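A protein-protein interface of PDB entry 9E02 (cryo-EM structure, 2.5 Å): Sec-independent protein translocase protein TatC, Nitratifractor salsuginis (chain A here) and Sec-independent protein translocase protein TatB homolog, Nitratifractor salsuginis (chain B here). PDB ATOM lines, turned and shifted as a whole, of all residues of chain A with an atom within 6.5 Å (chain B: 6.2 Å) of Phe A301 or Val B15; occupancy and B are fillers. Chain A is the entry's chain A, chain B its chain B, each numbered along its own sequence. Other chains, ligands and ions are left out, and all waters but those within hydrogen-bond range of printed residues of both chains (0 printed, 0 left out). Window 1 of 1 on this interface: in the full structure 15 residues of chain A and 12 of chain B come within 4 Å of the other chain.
Of the 18 printed residues of chain A, 7 touch a printed residue of chain B. Hydrophobic or aromatic side chains of chain A within 4 Å of the printed part of chain B: Ile A297, Val A298, Phe A301, Leu A302 and Ala A305. Printed residues of chain B that touch a printed residue of chain A: Glu B8, Val B11, Ile B12, Val B15, Ala B16, Phe B19 and Leu B20. Along chain B the printed residues that touch a printed residue of chain A span positions 8 to 20. Among the printed residues, 14 pairs touch across the chains. Among the printed residues, no Asp or Glu carboxylate lies within 4 Å of a Lys or Arg side-chain nitrogen of the other chain.
Of the printed residues of chain B, Ile A297 touches Val B15 (3.9 Å) and Phe B19 (3.7 Å). Phe A301 touches just these residues of chain B: Val B11 and Val B15. Of the printed residues of chain B, Leu A302 touches Ile B12 (3.6 Å). Printed residues of chain B within 4 Å of Gln A315: Glu B8 (3.4 Å), Val B11 (3.3 Å) and Ile B12 (3.5 Å). Ile A323 touches none of the printed residues of chain B. The nearest residue of chain A that does not touch Val B15 is Val A298 (4.2 Å). The nearest printed residue of chain A that does not touch Ala B16 is Lys A294 (6.2 Å).
NE2 of Gln A315 lies within hydrogen-bond range of O of Phe A301, 3.0 Å away.
Lys A294 touches Phe B19. Leu B20 touches Lys A294 (CD1 to O, 3.7 Å). CG1 of Val B15 touches CG1 of Ile A297, at 3.9 Å. Val A298 touches Ala B16 (CG2 to CA, 3.99 Å). CG2 of Val A298 touches CD1 of Leu B20 (3.6 Å). Phe A301 touches Val B11. Leu A302 touches Ile B12 (CD1 to CD1, 3.6 Å). CD1 of Ile B12 touches CB of Ala A305, at 3.9 Å. Gln A315 touches Glu B8 (CB to OE2, 3.4 Å). Gln A315 touches Ile B12.
The backbone carbonyl oxygen (O) of Ala A305 sits close to the side-chain carboxylate (OE1) of Glu B8, 3.2 Å away.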
ATOM      1  N   LYS A 294       3.914  14.639   7.265  1.00  0.00           N
ATOM      2  CA  LYS A 294       4.918  15.228   8.144  1.00  0.00           C
ATOM      3  C   LYS A 294       6.316  14.755   7.774  1.00  0.00           C
ATOM      4  O   LYS A 294       7.266  15.545   7.766  1.00  0.00           O
ATOM      5  CB  LYS A 294       4.606  14.886   9.597  1.00  0.00           C
ATOM      6  CG  LYS A 294       3.822  13.611   9.776  1.00  0.00           C
ATOM      7  CD  LYS A 294       3.174  13.546  11.140  1.00  0.00           C
ATOM      8  CE  LYS A 294       1.762  14.091  11.105  1.00  0.00           C
ATOM      9  NZ  LYS A 294       0.915  13.476  12.160  1.00  0.00           N
ATOM     10  N   ALA A 296       6.887  13.266   4.772  1.00  0.00           N
ATOM     11  CA  ALA A 296       7.007  13.507   3.342  1.00  0.00           C
ATOM     12  C   ALA A 296       7.601  14.874   3.060  1.00  0.00           C
ATOM     13  O   ALA A 296       8.402  15.024   2.138  1.00  0.00           O
ATOM     14  CB  ALA A 296       5.645  13.370   2.667  1.00  0.00           C
ATOM     15  N   ILE A 297       7.217  15.887   3.836  1.00  0.00           N
ATOM     16  CA  ILE A 297       7.727  17.231   3.591  1.00  0.00           C
ATOM     17  C   ILE A 297       9.212  17.315   3.930  1.00  0.00           C
ATOM     18  O   ILE A 297       9.983  17.989   3.237  1.00  0.00           O
ATOM     19  CB  ILE A 297       6.890  18.270   4.359  1.00  0.00           C
ATOM     20  CG1 ILE A 297       7.348  19.685   4.013  1.00  0.00           C
ATOM     21  CG2 ILE A 297       6.936  18.026   5.850  1.00  0.00           C
ATOM     22  CD1 ILE A 297       6.212  20.641   3.763  1.00  0.00           C
ATOM     23  N   VAL A 298       9.643  16.620   4.985  1.00  0.00           N
ATOM     24  CA  VAL A 298      11.062  16.588   5.321  1.00  0.00           C
ATOM     25  C   VAL A 298      11.852  15.896   4.219  1.00  0.00           C
ATOM     26  O   VAL A 298      12.922  16.364   3.811  1.00  0.00           O
ATOM     27  CB  VAL A 298      11.272  15.909   6.686  1.00  0.00           C
ATOM     28  CG1 VAL A 298      12.720  16.019   7.114  1.00  0.00           C
ATOM     29  CG2 VAL A 298      10.362  16.522   7.723  1.00  0.00           C
ATOM     30  N   ILE A 299      11.334  14.774   3.711  1.00  0.00           N
ATOM     31  CA  ILE A 299      12.005  14.083   2.614  1.00  0.00           C
ATOM     32  C   ILE A 299      12.008  14.948   1.358  1.00  0.00           C
ATOM     33  O   ILE A 299      12.963  14.931   0.577  1.00  0.00           O
ATOM     34  CB  ILE A 299      11.347  12.712   2.365  1.00  0.00           C
ATOM     35  CG1 ILE A 299      11.510  11.819   3.592  1.00  0.00           C
ATOM     36  CG2 ILE A 299      11.948  12.040   1.148  1.00  0.00           C
ATOM     37  CD1 ILE A 299      11.085  10.390   3.366  1.00  0.00           C
ATOM     38  N   ILE A 300      10.938  15.717   1.145  1.00  0.00           N
ATOM     39  CA  ILE A 300      10.856  16.604  -0.011  1.00  0.00           C
ATOM     40  C   ILE A 300      11.919  17.688   0.078  1.00  0.00           C
ATOM     41  O   ILE A 300      12.569  18.024  -0.918  1.00  0.00           O
ATOM     42  CB  ILE A 300       9.438  17.199  -0.126  1.00  0.00           C
ATOM     43  CG1 ILE A 300       8.519  16.254  -0.894  1.00  0.00           C
ATOM     44  CG2 ILE A 300       9.467  18.557  -0.797  1.00  0.00           C
ATOM     45  CD1 ILE A 300       7.059  16.492  -0.644  1.00  0.00           C
ATOM     46  N   PHE A 301      12.111  18.256   1.268  1.00  0.00           N
ATOM     47  CA  PHE A 301      13.138  19.278   1.434  1.00  0.00           C
ATOM     48  C   PHE A 301      14.533  18.684   1.300  1.00  0.00           C
ATOM     49  O   PHE A 301      15.436  19.324   0.751  1.00  0.00           O
ATOM     50  CB  PHE A 301      12.962  19.987   2.773  1.00  0.00           C
ATOM     51  CG  PHE A 301      12.051  21.176   2.704  1.00  0.00           C
ATOM     52  CD1 PHE A 301      10.685  21.026   2.852  1.00  0.00           C
ATOM     53  CD2 PHE A 301      12.557  22.439   2.469  1.00  0.00           C
ATOM     54  CE1 PHE A 301       9.848  22.113   2.780  1.00  0.00           C
ATOM     55  CE2 PHE A 301      11.722  23.527   2.395  1.00  0.00           C
ATOM     56  CZ  PHE A 301      10.365  23.362   2.552  1.00  0.00           C
ATOM     57  N   LEU A 302      14.723  17.450   1.771  1.00  0.00           N
ATOM     58  CA  LEU A 302      15.989  16.756   1.555  1.00  0.00           C
ATOM     59  C   LEU A 302      16.257  16.547   0.067  1.00  0.00           C
ATOM     60  O   LEU A 302      17.373  16.769  -0.417  1.00  0.00           O
ATOM     61  CB  LEU A 302      15.974  15.421   2.297  1.00  0.00           C
ATOM     62  CG  LEU A 302      17.300  14.717   2.570  1.00  0.00           C
ATOM     63  CD1 LEU A 302      18.374  15.705   2.985  1.00  0.00           C
ATOM     64  CD2 LEU A 302      17.114  13.648   3.631  1.00  0.00           C
ATOM     65  N   LEU A 303      15.232  16.127  -0.676  1.00  0.00           N
ATOM     66  CA  LEU A 303      15.368  15.938  -2.117  1.00  0.00           C
ATOM     67  C   LEU A 303      15.669  17.253  -2.820  1.00  0.00           C
ATOM     68  O   LEU A 303      16.485  17.298  -3.746  1.00  0.00           O
ATOM     69  CB  LEU A 303      14.092  15.319  -2.682  1.00  0.00           C
ATOM     70  CG  LEU A 303      14.092  13.824  -2.991  1.00  0.00           C
ATOM     71  CD1 LEU A 303      12.666  13.328  -3.135  1.00  0.00           C
ATOM     72  CD2 LEU A 303      14.892  13.537  -4.250  1.00  0.00           C
ATOM     73  N   ALA A 304      15.001  18.329  -2.405  1.00  0.00           N
ATOM     74  CA  ALA A 304      15.253  19.638  -2.993  1.00  0.00           C
ATOM     75  C   ALA A 304      16.679  20.096  -2.721  1.00  0.00           C
ATOM     76  O   ALA A 304      17.328  20.675  -3.596  1.00  0.00           O
ATOM     77  CB  ALA A 304      14.248  20.653  -2.456  1.00  0.00           C
ATOM     78  N   ALA A 305      17.180  19.849  -1.511  1.00  0.00           N
ATOM     79  CA  ALA A 305      18.571  20.163  -1.210  1.00  0.00           C
ATOM     80  C   ALA A 305      19.519  19.349  -2.079  1.00  0.00           C
ATOM     81  O   ALA A 305      20.527  19.869  -2.570  1.00  0.00           O
ATOM     82  CB  ALA A 305      18.854  19.920   0.270  1.00  0.00           C
ATOM     83  N   PHE A 306      19.212  18.067  -2.278  1.00  0.00           N
ATOM     84  CA  PHE A 306      20.073  17.211  -3.088  1.00  0.00           C
ATOM     85  C   PHE A 306      20.083  17.638  -4.551  1.00  0.00           C
ATOM     86  O   PHE A 306      21.128  17.594  -5.209  1.00  0.00           O
ATOM     87  CB  PHE A 306      19.627  15.755  -2.965  1.00  0.00           C
ATOM     88  CG  PHE A 306      20.203  15.042  -1.779  1.00  0.00           C
ATOM     89  CD1 PHE A 306      21.399  15.455  -1.218  1.00  0.00           C
ATOM     90  CD2 PHE A 306      19.548  13.957  -1.224  1.00  0.00           C
ATOM     91  CE1 PHE A 306      21.933  14.798  -0.126  1.00  0.00           C
ATOM     92  CE2 PHE A 306      20.074  13.296  -0.131  1.00  0.00           C
ATOM     93  CZ  PHE A 306      21.269  13.717   0.419  1.00  0.00           C
ATOM     94  N   GLN A 315      16.312  25.579  -3.012  1.00  0.00           N
ATOM     95  CA  GLN A 315      15.712  24.464  -2.292  1.00  0.00           C
ATOM     96  C   GLN A 315      14.217  24.674  -2.090  1.00  0.00           C
ATOM     97  O   GLN A 315      13.422  23.750  -2.288  1.00  0.00           O
ATOM     98  CB  GLN A 315      16.418  24.280  -0.950  1.00  0.00           C
ATOM     99  CG  GLN A 315      16.049  23.017  -0.217  1.00  0.00           C
ATOM    100  CD  GLN A 315      16.441  23.062   1.234  1.00  0.00           C
ATOM    101  OE1 GLN A 315      16.848  24.100   1.744  1.00  0.00           O
ATOM    102  NE2 GLN A 315      16.335  21.927   1.908  1.00  0.00           N
ATOM    103  N   LEU A 316      13.810  25.886  -1.710  1.00  0.00           N
ATOM    104  CA  LEU A 316      12.385  26.160  -1.543  1.00  0.00           C
ATOM    105  C   LEU A 316      11.659  26.152  -2.884  1.00  0.00           C
ATOM    106  O   LEU A 316      10.530  25.650  -2.987  1.00  0.00           O
ATOM    107  CB  LEU A 316      12.186  27.498  -0.832  1.00  0.00           C
ATOM    108  CG  LEU A 316      13.027  27.762   0.417  1.00  0.00           C
ATOM    109  CD1 LEU A 316      13.102  29.251   0.697  1.00  0.00           C
ATOM    110  CD2 LEU A 316      12.470  27.021   1.614  1.00  0.00           C
ATOM    111  N   ALA A 319      11.146  22.604  -3.623  1.00  0.00           N
ATOM    112  CA  ALA A 319      10.247  21.923  -2.701  1.00  0.00           C
ATOM    113  C   ALA A 319       8.791  22.255  -2.994  1.00  0.00           C
ATOM    114  O   ALA A 319       7.914  21.397  -2.839  1.00  0.00           O
ATOM    115  CB  ALA A 319      10.600  22.284  -1.262  1.00  0.00           C
ATOM    116  N   ALA A 320       8.511  23.492  -3.406  1.00  0.00           N
ATOM    117  CA  ALA A 320       7.123  23.881  -3.656  1.00  0.00           C
ATOM    118  C   ALA A 320       6.426  23.000  -4.689  1.00  0.00           C
ATOM    119  O   ALA A 320       5.306  22.531  -4.411  1.00  0.00           O
ATOM    120  CB  ALA A 320       7.069  25.361  -4.048  1.00  0.00           C
ATOM    121  N   LEU A 322       7.092  19.931  -5.450  1.00  0.00           N
ATOM    122  CA  LEU A 322       6.953  18.603  -4.866  1.00  0.00           C
ATOM    123  C   LEU A 322       5.804  18.553  -3.867  1.00  0.00           C
ATOM    124  O   LEU A 322       5.057  17.569  -3.819  1.00  0.00           O
ATOM    125  CB  LEU A 322       8.268  18.184  -4.214  1.00  0.00           C
ATOM    126  CG  LEU A 322       9.447  18.055  -5.178  1.00  0.00           C
ATOM    127  CD1 LEU A 322      10.696  17.589  -4.452  1.00  0.00           C
ATOM    128  CD2 LEU A 322       9.099  17.105  -6.308  1.00  0.00           C
ATOM    129  N   ILE A 323       5.635  19.611  -3.073  1.00  0.00           N
ATOM    130  CA  ILE A 323       4.503  19.675  -2.153  1.00  0.00           C
ATOM    131  C   ILE A 323       3.191  19.740  -2.924  1.00  0.00           C
ATOM    132  O   ILE A 323       2.199  19.096  -2.552  1.00  0.00           O
ATOM    133  CB  ILE A 323       4.665  20.869  -1.196  1.00  0.00           C
ATOM    134  CG1 ILE A 323       5.917  20.695  -0.338  1.00  0.00           C
ATOM    135  CG2 ILE A 323       3.443  21.013  -0.309  1.00  0.00           C
ATOM    136  CD1 ILE A 323       6.576  21.991   0.051  1.00  0.00           C
ATOM    137  N   GLU B   8      21.058  24.668   3.782  1.00  0.00           N
ATOM    138  CA  GLU B   8      20.034  23.708   3.384  1.00  0.00           C
ATOM    139  C   GLU B   8      19.789  22.674   4.477  1.00  0.00           C
ATOM    140  O   GLU B   8      18.643  22.288   4.728  1.00  0.00           O
ATOM    141  CB  GLU B   8      20.431  23.037   2.072  1.00  0.00           C
ATOM    142  CG  GLU B   8      20.408  23.973   0.880  1.00  0.00           C
ATOM    143  CD  GLU B   8      20.490  23.242  -0.443  1.00  0.00           C
ATOM    144  OE1 GLU B   8      21.283  22.286  -0.548  1.00  0.00           O
ATOM    145  OE2 GLU B   8      19.761  23.623  -1.381  1.00  0.00           O
ATOM    146  N   LEU B  10      20.200  23.307   7.634  1.00  0.00           N
ATOM    147  CA  LEU B  10      19.462  24.050   8.650  1.00  0.00           C
ATOM    148  C   LEU B  10      17.989  24.161   8.286  1.00  0.00           C
ATOM    149  O   LEU B  10      17.119  24.082   9.158  1.00  0.00           O
ATOM    150  CB  LEU B  10      20.076  25.435   8.840  1.00  0.00           C
ATOM    151  CG  LEU B  10      21.453  25.479   9.501  1.00  0.00           C
ATOM    152  CD1 LEU B  10      21.733  26.865  10.050  1.00  0.00           C
ATOM    153  CD2 LEU B  10      21.557  24.437  10.599  1.00  0.00           C
ATOM    154  N   VAL B  11      17.690  24.349   7.001  1.00  0.00           N
ATOM    155  CA  VAL B  11      16.301  24.433   6.564  1.00  0.00           C
ATOM    156  C   VAL B  11      15.602  23.089   6.736  1.00  0.00           C
ATOM    157  O   VAL B  11      14.434  23.031   7.132  1.00  0.00           O
ATOM    158  CB  VAL B  11      16.236  24.935   5.111  1.00  0.00           C
ATOM    159  CG1 VAL B  11      14.938  24.508   4.446  1.00  0.00           C
ATOM    160  CG2 VAL B  11      16.385  26.439   5.073  1.00  0.00           C
ATOM    161  N   ILE B  12      16.300  21.989   6.442  1.00  0.00           N
ATOM    162  CA  ILE B  12      15.718  20.665   6.655  1.00  0.00           C
ATOM    163  C   ILE B  12      15.434  20.442   8.134  1.00  0.00           C
ATOM    164  O   ILE B  12      14.388  19.897   8.507  1.00  0.00           O
ATOM    165  CB  ILE B  12      16.638  19.571   6.083  1.00  0.00           C
ATOM    166  CG1 ILE B  12      16.779  19.722   4.572  1.00  0.00           C
ATOM    167  CG2 ILE B  12      16.094  18.196   6.403  1.00  0.00           C
ATOM    168  CD1 ILE B  12      18.061  19.165   4.036  1.00  0.00           C
ATOM    169  N   ALA B  13      16.358  20.865   8.999  1.00  0.00           N
ATOM    170  CA  ALA B  13      16.128  20.776  10.437  1.00  0.00           C
ATOM    171  C   ALA B  13      14.941  21.632  10.864  1.00  0.00           C
ATOM    172  O   ALA B  13      14.144  21.223  11.713  1.00  0.00           O
ATOM    173  CB  ALA B  13      17.387  21.189  11.194  1.00  0.00           C
ATOM    174  N   LEU B  14      14.817  22.829  10.290  1.00  0.00           N
ATOM    175  CA  LEU B  14      13.689  23.703  10.590  1.00  0.00           C
ATOM    176  C   LEU B  14      12.372  23.048  10.202  1.00  0.00           C
ATOM    177  O   LEU B  14      11.394  23.093  10.955  1.00  0.00           O
ATOM    178  CB  LEU B  14      13.861  25.026   9.846  1.00  0.00           C
ATOM    179  CG  LEU B  14      13.221  26.295  10.397  1.00  0.00           C
ATOM    180  CD1 LEU B  14      14.077  26.862  11.508  1.00  0.00           C
ATOM    181  CD2 LEU B  14      13.052  27.302   9.286  1.00  0.00           C
ATOM    182  N   VAL B  15      12.332  22.438   9.017  1.00  0.00           N
ATOM    183  CA  VAL B  15      11.121  21.772   8.551  1.00  0.00           C
ATOM    184  C   VAL B  15      10.794  20.584   9.445  1.00  0.00           C
ATOM    185  O   VAL B  15       9.624  20.322   9.753  1.00  0.00           O
ATOM    186  CB  VAL B  15      11.281  21.356   7.077  1.00  0.00           C
ATOM    187  CG1 VAL B  15      10.087  20.548   6.610  1.00  0.00           C
ATOM    188  CG2 VAL B  15      11.463  22.579   6.208  1.00  0.00           C
ATOM    189  N   ALA B  16      11.821  19.852   9.880  1.00  0.00           N
ATOM    190  CA  ALA B  16      11.607  18.742  10.802  1.00  0.00           C
ATOM    191  C   ALA B  16      11.037  19.222  12.131  1.00  0.00           C
ATOM    192  O   ALA B  16      10.128  18.596  12.684  1.00  0.00           O
ATOM    193  CB  ALA B  16      12.915  17.989  11.024  1.00  0.00           C
ATOM    194  N   ILE B  17      11.560  20.325  12.664  1.00  0.00           N
ATOM    195  CA  ILE B  17      11.038  20.858  13.920  1.00  0.00           C
ATOM    196  C   ILE B  17       9.600  21.326  13.745  1.00  0.00           C
ATOM    197  O   ILE B  17       8.746  21.088  14.605  1.00  0.00           O
ATOM    198  CB  ILE B  17      11.937  21.992  14.446  1.00  0.00           C
ATOM    199  CG1 ILE B  17      13.346  21.480  14.722  1.00  0.00           C
ATOM    200  CG2 ILE B  17      11.356  22.590  15.708  1.00  0.00           C
ATOM    201  CD1 ILE B  17      14.213  22.462  15.459  1.00  0.00           C
ATOM    202  N   LEU B  18       9.312  21.999  12.633  1.00  0.00           N
ATOM    203  CA  LEU B  18       7.989  22.574  12.430  1.00  0.00           C
ATOM    204  C   LEU B  18       6.937  21.493  12.234  1.00  0.00           C
ATOM    205  O   LEU B  18       5.856  21.550  12.829  1.00  0.00           O
ATOM    206  CB  LEU B  18       8.017  23.517  11.229  1.00  0.00           C
ATOM    207  CG  LEU B  18       8.526  24.939  11.460  1.00  0.00           C
ATOM    208  CD1 LEU B  18       8.532  25.711  10.156  1.00  0.00           C
ATOM    209  CD2 LEU B  18       7.681  25.644  12.494  1.00  0.00           C
ATOM    210  N   PHE B  19       7.236  20.490  11.411  1.00  0.00           N
ATOM    211  CA  PHE B  19       6.208  19.547  10.992  1.00  0.00           C
ATOM    212  C   PHE B  19       6.157  18.293  11.844  1.00  0.00           C
ATOM    213  O   PHE B  19       5.077  17.715  12.008  1.00  0.00           O
ATOM    214  CB  PHE B  19       6.407  19.186   9.523  1.00  0.00           C
ATOM    215  CG  PHE B  19       5.927  20.249   8.587  1.00  0.00           C
ATOM    216  CD1 PHE B  19       4.593  20.333   8.247  1.00  0.00           C
ATOM    217  CD2 PHE B  19       6.802  21.193   8.082  1.00  0.00           C
ATOM    218  CE1 PHE B  19       4.146  21.317   7.402  1.00  0.00           C
ATOM    219  CE2 PHE B  19       6.361  22.181   7.238  1.00  0.00           C
ATOM    220  CZ  PHE B  19       5.031  22.245   6.897  1.00  0.00           C
ATOM    221  N   LEU B  20       7.284  17.854  12.399  1.00  0.00           N
ATOM    222  CA  LEU B  20       7.230  16.767  13.365  1.00  0.00           C
ATOM    223  C   LEU B  20       6.850  17.302  14.743  1.00  0.00           C
ATOM    224  O   LEU B  20       5.796  16.957  15.283  1.00  0.00           O
ATOM    225  CB  LEU B  20       8.563  16.023  13.394  1.00  0.00           C
ATOM    226  CG  LEU B  20       8.732  14.949  12.317  1.00  0.00           C
ATOM    227  CD1 LEU B  20       9.025  15.553  10.971  1.00  0.00           C
ATOM    228  CD2 LEU B  20       9.845  14.010  12.704  1.00  0.00           C
